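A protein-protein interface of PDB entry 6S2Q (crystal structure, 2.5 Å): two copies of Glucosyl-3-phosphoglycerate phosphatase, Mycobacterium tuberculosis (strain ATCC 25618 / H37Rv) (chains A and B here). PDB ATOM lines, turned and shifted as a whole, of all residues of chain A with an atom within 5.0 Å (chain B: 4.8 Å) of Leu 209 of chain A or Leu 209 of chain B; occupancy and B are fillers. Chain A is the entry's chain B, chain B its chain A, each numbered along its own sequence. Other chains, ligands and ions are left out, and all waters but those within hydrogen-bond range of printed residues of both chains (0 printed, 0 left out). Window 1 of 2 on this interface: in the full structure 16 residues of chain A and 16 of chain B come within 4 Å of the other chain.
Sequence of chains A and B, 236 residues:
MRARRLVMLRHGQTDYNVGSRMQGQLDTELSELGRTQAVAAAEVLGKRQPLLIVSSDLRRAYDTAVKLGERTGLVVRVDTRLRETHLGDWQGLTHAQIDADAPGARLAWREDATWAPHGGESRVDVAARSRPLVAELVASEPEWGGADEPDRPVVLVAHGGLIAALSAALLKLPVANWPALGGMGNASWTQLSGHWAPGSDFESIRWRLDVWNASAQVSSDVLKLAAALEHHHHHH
Printed residues of chain B that touch a printed residue of chain A: Ala 180, Leu 181, Gly 182, Arg 208, Leu 209, Asp 210, Val 211 and Trp 212.
Hydrophobic or aromatic side chains of chain B within 4 Å of the printed part of chain A: Leu 181, Leu 209, Val 211 and Trp 212.
Of the 13 printed residues of chain A, 7 touch a printed residue of chain B.
Hydrophobic or aromatic side chains of chain A that line the printed part of chain B: Leu 209, Val 211 and Trp 212.
Among the printed residues, no Asp or Glu carboxylate lies within 4 Å of a Lys or Arg side-chain nitrogen of the other chain.
Ala 180 of chain A touches Leu 209 of chain B, and with the chains exchanged Leu 209 of chain A touches Ala 180 of chain B.
Gly 182 of chain A touches Leu 209 of chain B, and with the chains exchanged Leu 209 of chain A touches Gly 182 of chain B.
Val 211 of chain A touches Trp 212 of chain B, and with the chains exchanged Trp 212 of chain A touches Val 211 of chain B.
Trp 212 of chain A touches its own counterpart, Trp 212 of chain B.
13 positions are printed for both chains.
The backbone carbonyl oxygen (O) of Val 211 of chain A is in hydrogen-bond range of the backbone NH (N) of Gln 191 of chain A (2.7 Å).
The indole nitrogen of Trp 212 of chain A lies close to the backbone carbonyl oxygen of Gly 182 of chain A (3.5 Å).
The side-chain amide nitrogen (NE2) of Gln 191 of chain B sits at hydrogen-bond distance from the side-chain carboxylate (OD2) of Asp 210 of chain B, at 2.6 Å.
The side-chain amide nitrogen (NE2) of Gln 191 of chain A lies within hydrogen-bond range of the side-chain carboxylate (OD2) of Asp 210 of chain A (2.5 Å).
NE1 of Trp 212 of chain B sits close to O of Gly 182 of chain B, at 3.3 Å.
The backbone NH (N) of Gln 191 of chain B sits at hydrogen-bond distance from the backbone carbonyl oxygen (O) of Val 211 of chain B, at 2.8 Å.
Arg 208 of chain B touches Ala 180 of chain A.
CA of Gly 182 of chain A touches CD of Arg 208 of chain B, 3.5 Å away.
Arg 208 of chain A touches Ala 180 of chain B.
Arg 208 of chain A touches Gly 182 of chain B.
Leu 209 of chain A touches Leu 181 of chain B.
CD2 of Leu 209 of chain A touches CD2 of Leu 209 of chain B, at 3.9 Å.
Trp 212 of chain B touches Leu 209 of chain A (NE1 to O, 3.7 Å).
Val 211 of chain A touches Trp 212 of chain B.
Leu 209 of chain B touches Trp 212 of chain A.
Trp 212 of chain A touches Asp 210 of chain B.
N of Trp 212 of chain B lies within hydrogen-bond range of O of Trp 212 of chain A, at 2.8 Å.
N of Gly 182 of chain B sits at hydrogen-bond distance from O of Leu 209 of chain A (2.7 Å).
The backbone carbonyl oxygen of Ala 180 of chain B is in hydrogen-bond range of the backbone NH of Leu 209 of chain A, at 2.7 Å.
N of Leu 209 of chain B sits at hydrogen-bond distance from O of Ala 180 of chain A (2.6 Å).
O of Leu 209 of chain B is in hydrogen-bond range of N of Gly 182 of chain A, at 3.0 Å.
Of the printed residues of chain B, Gly 182 of chain A touches Arg 208 and Leu 209.
Of chain B, only Ala 180 (2.7 Å), Leu 181 (3.8 Å), Gly 182 (2.7 Å), Leu 209 (3.9 Å) and Trp 212 (3.7 Å) come within 4 Å of Leu 209 of chain A.
Printed residues of chain B within 4 Å of Trp 212 of chain A: Leu 209 (3.6 Å), Asp 210 (3.4 Å), Val 211 (3.4 Å) and Trp 212 (2.8 Å).
Printed residues of chain A within 4 Å of Leu 181 of chain B: Leu 209.
Printed residues of chain A within 4 Å of Arg 208 of chain B: Ala 180 (3.5 Å) and Gly 182 (3.5 Å).
Leu 209 of chain B touches just these residues of chain A: Ala 180, Gly 182, Leu 209 and Trp 212.
Printed residues of chain A within 4 Å of Asp 210 of chain B: Trp 212 (3.4 Å).
The nearest residue of chain A that does not touch Leu 209 of chain B is Leu 181 of chain A (4.1 Å).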
ATOM      1  N   LEU A 171      -3.260   3.700  19.244  1.00  0.00           N
ATOM      2  CA  LEU A 171      -3.779   2.561  18.494  1.00  0.00           C
ATOM      3  C   LEU A 171      -2.782   1.426  18.404  1.00  0.00           C
ATOM      4  O   LEU A 171      -3.104   0.395  17.809  1.00  0.00           O
ATOM      5  CB  LEU A 171      -4.187   2.982  17.082  1.00  0.00           C
ATOM      6  CG  LEU A 171      -5.335   3.986  17.045  1.00  0.00           C
ATOM      7  CD1 LEU A 171      -5.500   4.655  15.678  1.00  0.00           C
ATOM      8  CD2 LEU A 171      -6.613   3.273  17.432  1.00  0.00           C
ATOM      9  N   ALA A 180      -0.074   5.720   7.449  1.00  0.00           N
ATOM     10  CA  ALA A 180      -1.426   5.505   6.954  1.00  0.00           C
ATOM     11  C   ALA A 180      -2.372   6.613   7.391  1.00  0.00           C
ATOM     12  O   ALA A 180      -3.318   6.942   6.660  1.00  0.00           O
ATOM     13  CB  ALA A 180      -1.947   4.154   7.422  1.00  0.00           C
ATOM     14  N   LEU A 181      -2.125   7.230   8.546  1.00  0.00           N
ATOM     15  CA  LEU A 181      -3.001   8.298   9.025  1.00  0.00           C
ATOM     16  C   LEU A 181      -2.642   9.610   8.335  1.00  0.00           C
ATOM     17  O   LEU A 181      -1.687  10.281   8.718  1.00  0.00           O
ATOM     18  CB  LEU A 181      -2.899   8.443  10.537  1.00  0.00           C
ATOM     19  CG  LEU A 181      -3.427   7.294  11.385  1.00  0.00           C
ATOM     20  CD1 LEU A 181      -3.151   7.559  12.854  1.00  0.00           C
ATOM     21  CD2 LEU A 181      -4.919   7.112  11.139  1.00  0.00           C
ATOM     22  N   GLY A 182      -3.455  10.013   7.358  1.00  0.00           N
ATOM     23  CA  GLY A 182      -3.229  11.246   6.637  1.00  0.00           C
ATOM     24  C   GLY A 182      -3.475  12.470   7.504  1.00  0.00           C
ATOM     25  O   GLY A 182      -3.766  12.377   8.687  1.00  0.00           O
ATOM     26  N   THR A 190     -10.695  14.302  15.800  1.00  0.00           N
ATOM     27  CA  THR A 190     -10.475  12.864  15.808  1.00  0.00           C
ATOM     28  C   THR A 190     -10.926  12.342  17.164  1.00  0.00           C
ATOM     29  O   THR A 190     -10.799  13.029  18.179  1.00  0.00           O
ATOM     30  CB  THR A 190      -8.975  12.515  15.551  1.00  0.00           C
ATOM     31  OG1 THR A 190      -8.658  12.750  14.179  1.00  0.00           O
ATOM     32  CG2 THR A 190      -8.646  11.073  15.903  1.00  0.00           C
ATOM     33  N   GLN A 191     -11.464  11.131  17.190  1.00  0.00           N
ATOM     34  CA  GLN A 191     -11.903  10.551  18.450  1.00  0.00           C
ATOM     35  C   GLN A 191     -11.459   9.100  18.552  1.00  0.00           C
ATOM     36  O   GLN A 191     -11.835   8.263  17.722  1.00  0.00           O
ATOM     37  CB  GLN A 191     -13.421  10.638  18.605  1.00  0.00           C
ATOM     38  CG  GLN A 191     -13.850  10.049  19.914  1.00  0.00           C
ATOM     39  CD  GLN A 191     -15.342   9.922  20.050  1.00  0.00           C
ATOM     40  OE1 GLN A 191     -16.062  10.922  20.152  1.00  0.00           O
ATOM     41  NE2 GLN A 191     -15.823   8.683  20.076  1.00  0.00           N
ATOM     42  N   LEU A 192     -10.728   8.792  19.612  1.00  0.00           N
ATOM     43  CA  LEU A 192     -10.412   7.429  19.988  1.00  0.00           C
ATOM     44  C   LEU A 192     -11.210   7.125  21.246  1.00  0.00           C
ATOM     45  O   LEU A 192     -11.522   8.025  22.028  1.00  0.00           O
ATOM     46  CB  LEU A 192      -8.917   7.255  20.279  1.00  0.00           C
ATOM     47  CG  LEU A 192      -7.853   7.720  19.259  1.00  0.00           C
ATOM     48  CD1 LEU A 192      -6.437   7.338  19.718  1.00  0.00           C
ATOM     49  CD2 LEU A 192      -8.071   7.291  17.815  1.00  0.00           C
ATOM     50  N   TRP A 207      -7.131   1.015  22.488  1.00  0.00           N
ATOM     51  CA  TRP A 207      -7.738   2.198  21.894  1.00  0.00           C
ATOM     52  C   TRP A 207      -8.309   1.854  20.533  1.00  0.00           C
ATOM     53  O   TRP A 207      -7.731   1.065  19.782  1.00  0.00           O
ATOM     54  CB  TRP A 207      -6.734   3.345  21.757  1.00  0.00           C
ATOM     55  CG  TRP A 207      -6.345   3.890  23.073  1.00  0.00           C
ATOM     56  CD1 TRP A 207      -5.259   3.545  23.823  1.00  0.00           C
ATOM     57  CD2 TRP A 207      -7.088   4.831  23.848  1.00  0.00           C
ATOM     58  NE1 TRP A 207      -5.270   4.235  25.010  1.00  0.00           N
ATOM     59  CE2 TRP A 207      -6.383   5.034  25.047  1.00  0.00           C
ATOM     60  CE3 TRP A 207      -8.287   5.522  23.645  1.00  0.00           C
ATOM     61  CZ2 TRP A 207      -6.829   5.914  26.033  1.00  0.00           C
ATOM     62  CZ3 TRP A 207      -8.730   6.390  24.624  1.00  0.00           C
ATOM     63  CH2 TRP A 207      -8.000   6.584  25.800  1.00  0.00           C
ATOM     64  N   ARG A 208      -9.464   2.426  20.236  1.00  0.00           N
ATOM     65  CA  ARG A 208     -10.131   2.198  18.969  1.00  0.00           C
ATOM     66  C   ARG A 208     -10.298   3.542  18.277  1.00  0.00           C
ATOM     67  O   ARG A 208     -10.609   4.546  18.920  1.00  0.00           O
ATOM     68  CB  ARG A 208     -11.504   1.546  19.162  1.00  0.00           C
ATOM     69  CG  ARG A 208     -11.784   0.420  18.203  1.00  0.00           C
ATOM     70  CD  ARG A 208     -13.251   0.005  18.221  1.00  0.00           C
ATOM     71  NE  ARG A 208     -13.733  -0.674  19.414  1.00  0.00           N
ATOM     72  CZ  ARG A 208     -15.034  -0.826  19.664  1.00  0.00           C
ATOM     73  NH1 ARG A 208     -15.927  -0.337  18.798  1.00  0.00           N
ATOM     74  NH2 ARG A 208     -15.448  -1.459  20.763  1.00  0.00           N
ATOM     75  N   LEU A 209     -10.108   3.556  16.968  1.00  0.00           N
ATOM     76  CA  LEU A 209     -10.354   4.755  16.181  1.00  0.00           C
ATOM     77  C   LEU A 209     -11.855   4.879  15.936  1.00  0.00           C
ATOM     78  O   LEU A 209     -12.442   4.071  15.208  1.00  0.00           O
ATOM     79  CB  LEU A 209      -9.588   4.660  14.870  1.00  0.00           C
ATOM     80  CG  LEU A 209      -9.696   5.820  13.890  1.00  0.00           C
ATOM     81  CD1 LEU A 209      -9.192   7.124  14.495  1.00  0.00           C
ATOM     82  CD2 LEU A 209      -8.889   5.476  12.663  1.00  0.00           C
ATOM     83  N   ASP A 210     -12.498   5.867  16.565  1.00  0.00           N
ATOM     84  CA  ASP A 210     -13.922   6.052  16.306  1.00  0.00           C
ATOM     85  C   ASP A 210     -14.151   6.954  15.109  1.00  0.00           C
ATOM     86  O   ASP A 210     -14.990   6.658  14.247  1.00  0.00           O
ATOM     87  CB  ASP A 210     -14.643   6.664  17.505  1.00  0.00           C
ATOM     88  CG  ASP A 210     -14.587   5.798  18.721  1.00  0.00           C
ATOM     89  OD1 ASP A 210     -14.275   4.590  18.587  1.00  0.00           O
ATOM     90  OD2 ASP A 210     -14.942   6.314  19.798  1.00  0.00           O
ATOM     91  N   VAL A 211     -13.450   8.090  15.099  1.00  0.00           N
ATOM     92  CA  VAL A 211     -13.611   9.133  14.098  1.00  0.00           C
ATOM     93  C   VAL A 211     -12.230   9.682  13.801  1.00  0.00           C
ATOM     94  O   VAL A 211     -11.485  10.004  14.732  1.00  0.00           O
ATOM     95  CB  VAL A 211     -14.525  10.269  14.599  1.00  0.00           C
ATOM     96  CG1 VAL A 211     -14.655  11.341  13.545  1.00  0.00           C
ATOM     97  CG2 VAL A 211     -15.875   9.747  15.032  1.00  0.00           C
ATOM     98  N   TRP A 212     -11.887   9.807  12.522  1.00  0.00           N
ATOM     99  CA  TRP A 212     -10.647  10.460  12.115  1.00  0.00           C
ATOM    100  C   TRP A 212     -10.963  11.581  11.145  1.00  0.00           C
ATOM    101  O   TRP A 212     -11.540  11.334  10.085  1.00  0.00           O
ATOM    102  CB  TRP A 212      -9.663   9.488  11.472  1.00  0.00           C
ATOM    103  CG  TRP A 212      -8.396  10.173  10.957  1.00  0.00           C
ATOM    104  CD1 TRP A 212      -8.122  10.538   9.666  1.00  0.00           C
ATOM    105  CD2 TRP A 212      -7.257  10.561  11.728  1.00  0.00           C
ATOM    106  NE1 TRP A 212      -6.874  11.111   9.587  1.00  0.00           N
ATOM    107  CE2 TRP A 212      -6.325  11.146  10.839  1.00  0.00           C
ATOM    108  CE3 TRP A 212      -6.931  10.477  13.084  1.00  0.00           C
ATOM    109  CZ2 TRP A 212      -5.098  11.649  11.263  1.00  0.00           C
ATOM    110  CZ3 TRP A 212      -5.695  10.974  13.503  1.00  0.00           C
ATOM    111  CH2 TRP A 212      -4.797  11.552  12.592  1.00  0.00           C
ATOM    112  N   LEU B 171      -5.024  -0.049   3.102  1.00  0.00           N
ATOM    113  CA  LEU B 171      -3.976   0.554   3.912  1.00  0.00           C
ATOM    114  C   LEU B 171      -2.828  -0.407   4.205  1.00  0.00           C
ATOM    115  O   LEU B 171      -1.825   0.016   4.787  1.00  0.00           O
ATOM    116  CB  LEU B 171      -4.573   1.049   5.227  1.00  0.00           C
ATOM    117  CG  LEU B 171      -5.644   2.132   5.070  1.00  0.00           C
ATOM    118  CD1 LEU B 171      -6.365   2.395   6.358  1.00  0.00           C
ATOM    119  CD2 LEU B 171      -5.055   3.427   4.499  1.00  0.00           C
ATOM    120  N   ALA B 180      -8.541  -2.055  14.984  1.00  0.00           N
ATOM    121  CA  ALA B 180      -8.382  -0.687  15.469  1.00  0.00           C
ATOM    122  C   ALA B 180      -9.439   0.249  14.896  1.00  0.00           C
ATOM    123  O   ALA B 180      -9.779   1.259  15.523  1.00  0.00           O
ATOM    124  CB  ALA B 180      -6.973  -0.171  15.154  1.00  0.00           C
ATOM    125  N   LEU B 181      -9.976  -0.067  13.731  1.00  0.00           N
ATOM    126  CA  LEU B 181     -10.953   0.793  13.067  1.00  0.00           C
ATOM    127  C   LEU B 181     -12.330   0.571  13.674  1.00  0.00           C
ATOM    128  O   LEU B 181     -13.016  -0.402  13.319  1.00  0.00           O
ATOM    129  CB  LEU B 181     -11.008   0.459  11.584  1.00  0.00           C
ATOM    130  CG  LEU B 181      -9.746   0.673  10.767  1.00  0.00           C
ATOM    131  CD1 LEU B 181      -9.983   0.180   9.348  1.00  0.00           C
ATOM    132  CD2 LEU B 181      -9.326   2.126  10.792  1.00  0.00           C
ATOM    133  N   GLY B 182     -12.790   1.526  14.497  1.00  0.00           N
ATOM    134  CA  GLY B 182     -14.102   1.416  15.123  1.00  0.00           C
ATOM    135  C   GLY B 182     -15.220   1.457  14.086  1.00  0.00           C
ATOM    136  O   GLY B 182     -14.986   1.599  12.893  1.00  0.00           O
ATOM    137  N   THR B 190     -16.075   7.338   4.770  1.00  0.00           N
ATOM    138  CA  THR B 190     -14.644   7.246   4.962  1.00  0.00           C
ATOM    139  C   THR B 190     -13.969   7.585   3.640  1.00  0.00           C
ATOM    140  O   THR B 190     -14.536   7.359   2.561  1.00  0.00           O
ATOM    141  CB  THR B 190     -14.281   5.863   5.444  1.00  0.00           C
ATOM    142  OG1 THR B 190     -14.686   5.742   6.809  1.00  0.00           O
ATOM    143  CG2 THR B 190     -12.780   5.598   5.324  1.00  0.00           C
ATOM    144  N   GLN B 191     -12.787   8.197   3.715  1.00  0.00           N
ATOM    145  CA  GLN B 191     -12.080   8.561   2.502  1.00  0.00           C
ATOM    146  C   GLN B 191     -10.621   8.164   2.614  1.00  0.00           C
ATOM    147  O   GLN B 191      -9.941   8.517   3.581  1.00  0.00           O
ATOM    148  CB  GLN B 191     -12.184  10.052   2.210  1.00  0.00           C
ATOM    149  CG  GLN B 191     -11.498  10.422   0.926  1.00  0.00           C
ATOM    150  CD  GLN B 191     -11.371  11.908   0.732  1.00  0.00           C
ATOM    151  OE1 GLN B 191     -12.363  12.647   0.763  1.00  0.00           O
ATOM    152  NE2 GLN B 191     -10.132  12.368   0.525  1.00  0.00           N
ATOM    153  N   LEU B 192     -10.158   7.406   1.636  1.00  0.00           N
ATOM    154  CA  LEU B 192      -8.758   7.099   1.412  1.00  0.00           C
ATOM    155  C   LEU B 192      -8.311   7.832   0.154  1.00  0.00           C
ATOM    156  O   LEU B 192      -9.123   8.113  -0.728  1.00  0.00           O
ATOM    157  CB  LEU B 192      -8.559   5.591   1.232  1.00  0.00           C
ATOM    158  CG  LEU B 192      -8.683   4.528   2.327  1.00  0.00           C
ATOM    159  CD1 LEU B 192      -9.900   4.685   3.173  1.00  0.00           C
ATOM    160  CD2 LEU B 192      -8.751   3.160   1.662  1.00  0.00           C
ATOM    161  N   TRP B 207      -2.000   3.826  -0.049  1.00  0.00           N
ATOM    162  CA  TRP B 207      -3.265   4.393   0.374  1.00  0.00           C
ATOM    163  C   TRP B 207      -3.089   5.029   1.739  1.00  0.00           C
ATOM    164  O   TRP B 207      -2.412   4.475   2.608  1.00  0.00           O
ATOM    165  CB  TRP B 207      -4.348   3.320   0.406  1.00  0.00           C
ATOM    166  CG  TRP B 207      -4.687   2.818  -0.949  1.00  0.00           C
ATOM    167  CD1 TRP B 207      -4.138   1.748  -1.586  1.00  0.00           C
ATOM    168  CD2 TRP B 207      -5.670   3.354  -1.834  1.00  0.00           C
ATOM    169  NE1 TRP B 207      -4.706   1.592  -2.822  1.00  0.00           N
ATOM    170  CE2 TRP B 207      -5.653   2.564  -3.001  1.00  0.00           C
ATOM    171  CE3 TRP B 207      -6.563   4.428  -1.754  1.00  0.00           C
ATOM    172  CZ2 TRP B 207      -6.496   2.811  -4.086  1.00  0.00           C
ATOM    173  CZ3 TRP B 207      -7.398   4.675  -2.826  1.00  0.00           C
ATOM    174  CH2 TRP B 207      -7.363   3.868  -3.980  1.00  0.00           C
ATOM    175  N   ARG B 208      -3.707   6.194   1.914  1.00  0.00           N
ATOM    176  CA  ARG B 208      -3.645   6.982   3.138  1.00  0.00           C
ATOM    177  C   ARG B 208      -5.070   7.170   3.631  1.00  0.00           C
ATOM    178  O   ARG B 208      -5.970   7.381   2.823  1.00  0.00           O
ATOM    179  CB  ARG B 208      -2.999   8.344   2.864  1.00  0.00           C
ATOM    180  CG  ARG B 208      -2.010   8.791   3.891  1.00  0.00           C
ATOM    181  CD  ARG B 208      -1.576  10.241   3.661  1.00  0.00           C
ATOM    182  NE  ARG B 208      -0.727  10.497   2.491  1.00  0.00           N
ATOM    183  CZ  ARG B 208       0.593  10.317   2.467  1.00  0.00           C
ATOM    184  NH1 ARG B 208       1.221   9.849   3.549  1.00  0.00           N
ATOM    185  NH2 ARG B 208       1.286  10.608   1.365  1.00  0.00           N
ATOM    186  N   LEU B 209      -5.296   7.100   4.939  1.00  0.00           N
ATOM    187  CA  LEU B 209      -6.637   7.346   5.472  1.00  0.00           C
ATOM    188  C   LEU B 209      -6.864   8.850   5.593  1.00  0.00           C
ATOM    189  O   LEU B 209      -6.224   9.514   6.411  1.00  0.00           O
ATOM    190  CB  LEU B 209      -6.828   6.653   6.818  1.00  0.00           C
ATOM    191  CG  LEU B 209      -8.216   6.803   7.462  1.00  0.00           C
ATOM    192  CD1 LEU B 209      -9.328   6.232   6.552  1.00  0.00           C
ATOM    193  CD2 LEU B 209      -8.291   6.152   8.853  1.00  0.00           C
ATOM    194  N   ASP B 210      -7.769   9.395   4.775  1.00  0.00           N
ATOM    195  CA  ASP B 210      -8.062  10.824   4.850  1.00  0.00           C
ATOM    196  C   ASP B 210      -9.109  11.114   5.912  1.00  0.00           C
ATOM    197  O   ASP B 210      -8.926  12.024   6.733  1.00  0.00           O
ATOM    198  CB  ASP B 210      -8.544  11.364   3.504  1.00  0.00           C
ATOM    199  CG  ASP B 210      -7.502  11.241   2.404  1.00  0.00           C
ATOM    200  OD1 ASP B 210      -6.304  11.103   2.716  1.00  0.00           O
ATOM    201  OD2 ASP B 210      -7.893  11.288   1.214  1.00  0.00           O
ATOM    202  N   VAL B 211     -10.208  10.361   5.904  1.00  0.00           N
ATOM    203  CA  VAL B 211     -11.340  10.578   6.796  1.00  0.00           C
ATOM    204  C   VAL B 211     -11.868   9.214   7.222  1.00  0.00           C
ATOM    205  O   VAL B 211     -11.995   8.309   6.389  1.00  0.00           O
ATOM    206  CB  VAL B 211     -12.471  11.376   6.109  1.00  0.00           C
ATOM    207  CG1 VAL B 211     -13.633  11.572   7.060  1.00  0.00           C
ATOM    208  CG2 VAL B 211     -11.977  12.686   5.539  1.00  0.00           C
ATOM    209  N   TRP B 212     -12.162   9.048   8.514  1.00  0.00           N
ATOM    210  CA  TRP B 212     -12.825   7.842   8.990  1.00  0.00           C
ATOM    211  C   TRP B 212     -14.093   8.219   9.745  1.00  0.00           C
ATOM    212  O   TRP B 212     -14.033   8.878  10.786  1.00  0.00           O
ATOM    213  CB  TRP B 212     -11.905   6.990   9.865  1.00  0.00           C
ATOM    214  CG  TRP B 212     -12.615   5.793  10.379  1.00  0.00           C
ATOM    215  CD1 TRP B 212     -13.161   5.640  11.617  1.00  0.00           C
ATOM    216  CD2 TRP B 212     -12.940   4.594   9.642  1.00  0.00           C
ATOM    217  NE1 TRP B 212     -13.768   4.404  11.719  1.00  0.00           N
ATOM    218  CE2 TRP B 212     -13.656   3.745  10.521  1.00  0.00           C
ATOM    219  CE3 TRP B 212     -12.667   4.145   8.346  1.00  0.00           C
ATOM    220  CZ2 TRP B 212     -14.121   2.458  10.135  1.00  0.00           C
ATOM    221  CZ3 TRP B 212     -13.143   2.869   7.951  1.00  0.00           C
ATOM    222  CH2 TRP B 212     -13.866   2.048   8.847  1.00  0.00           C
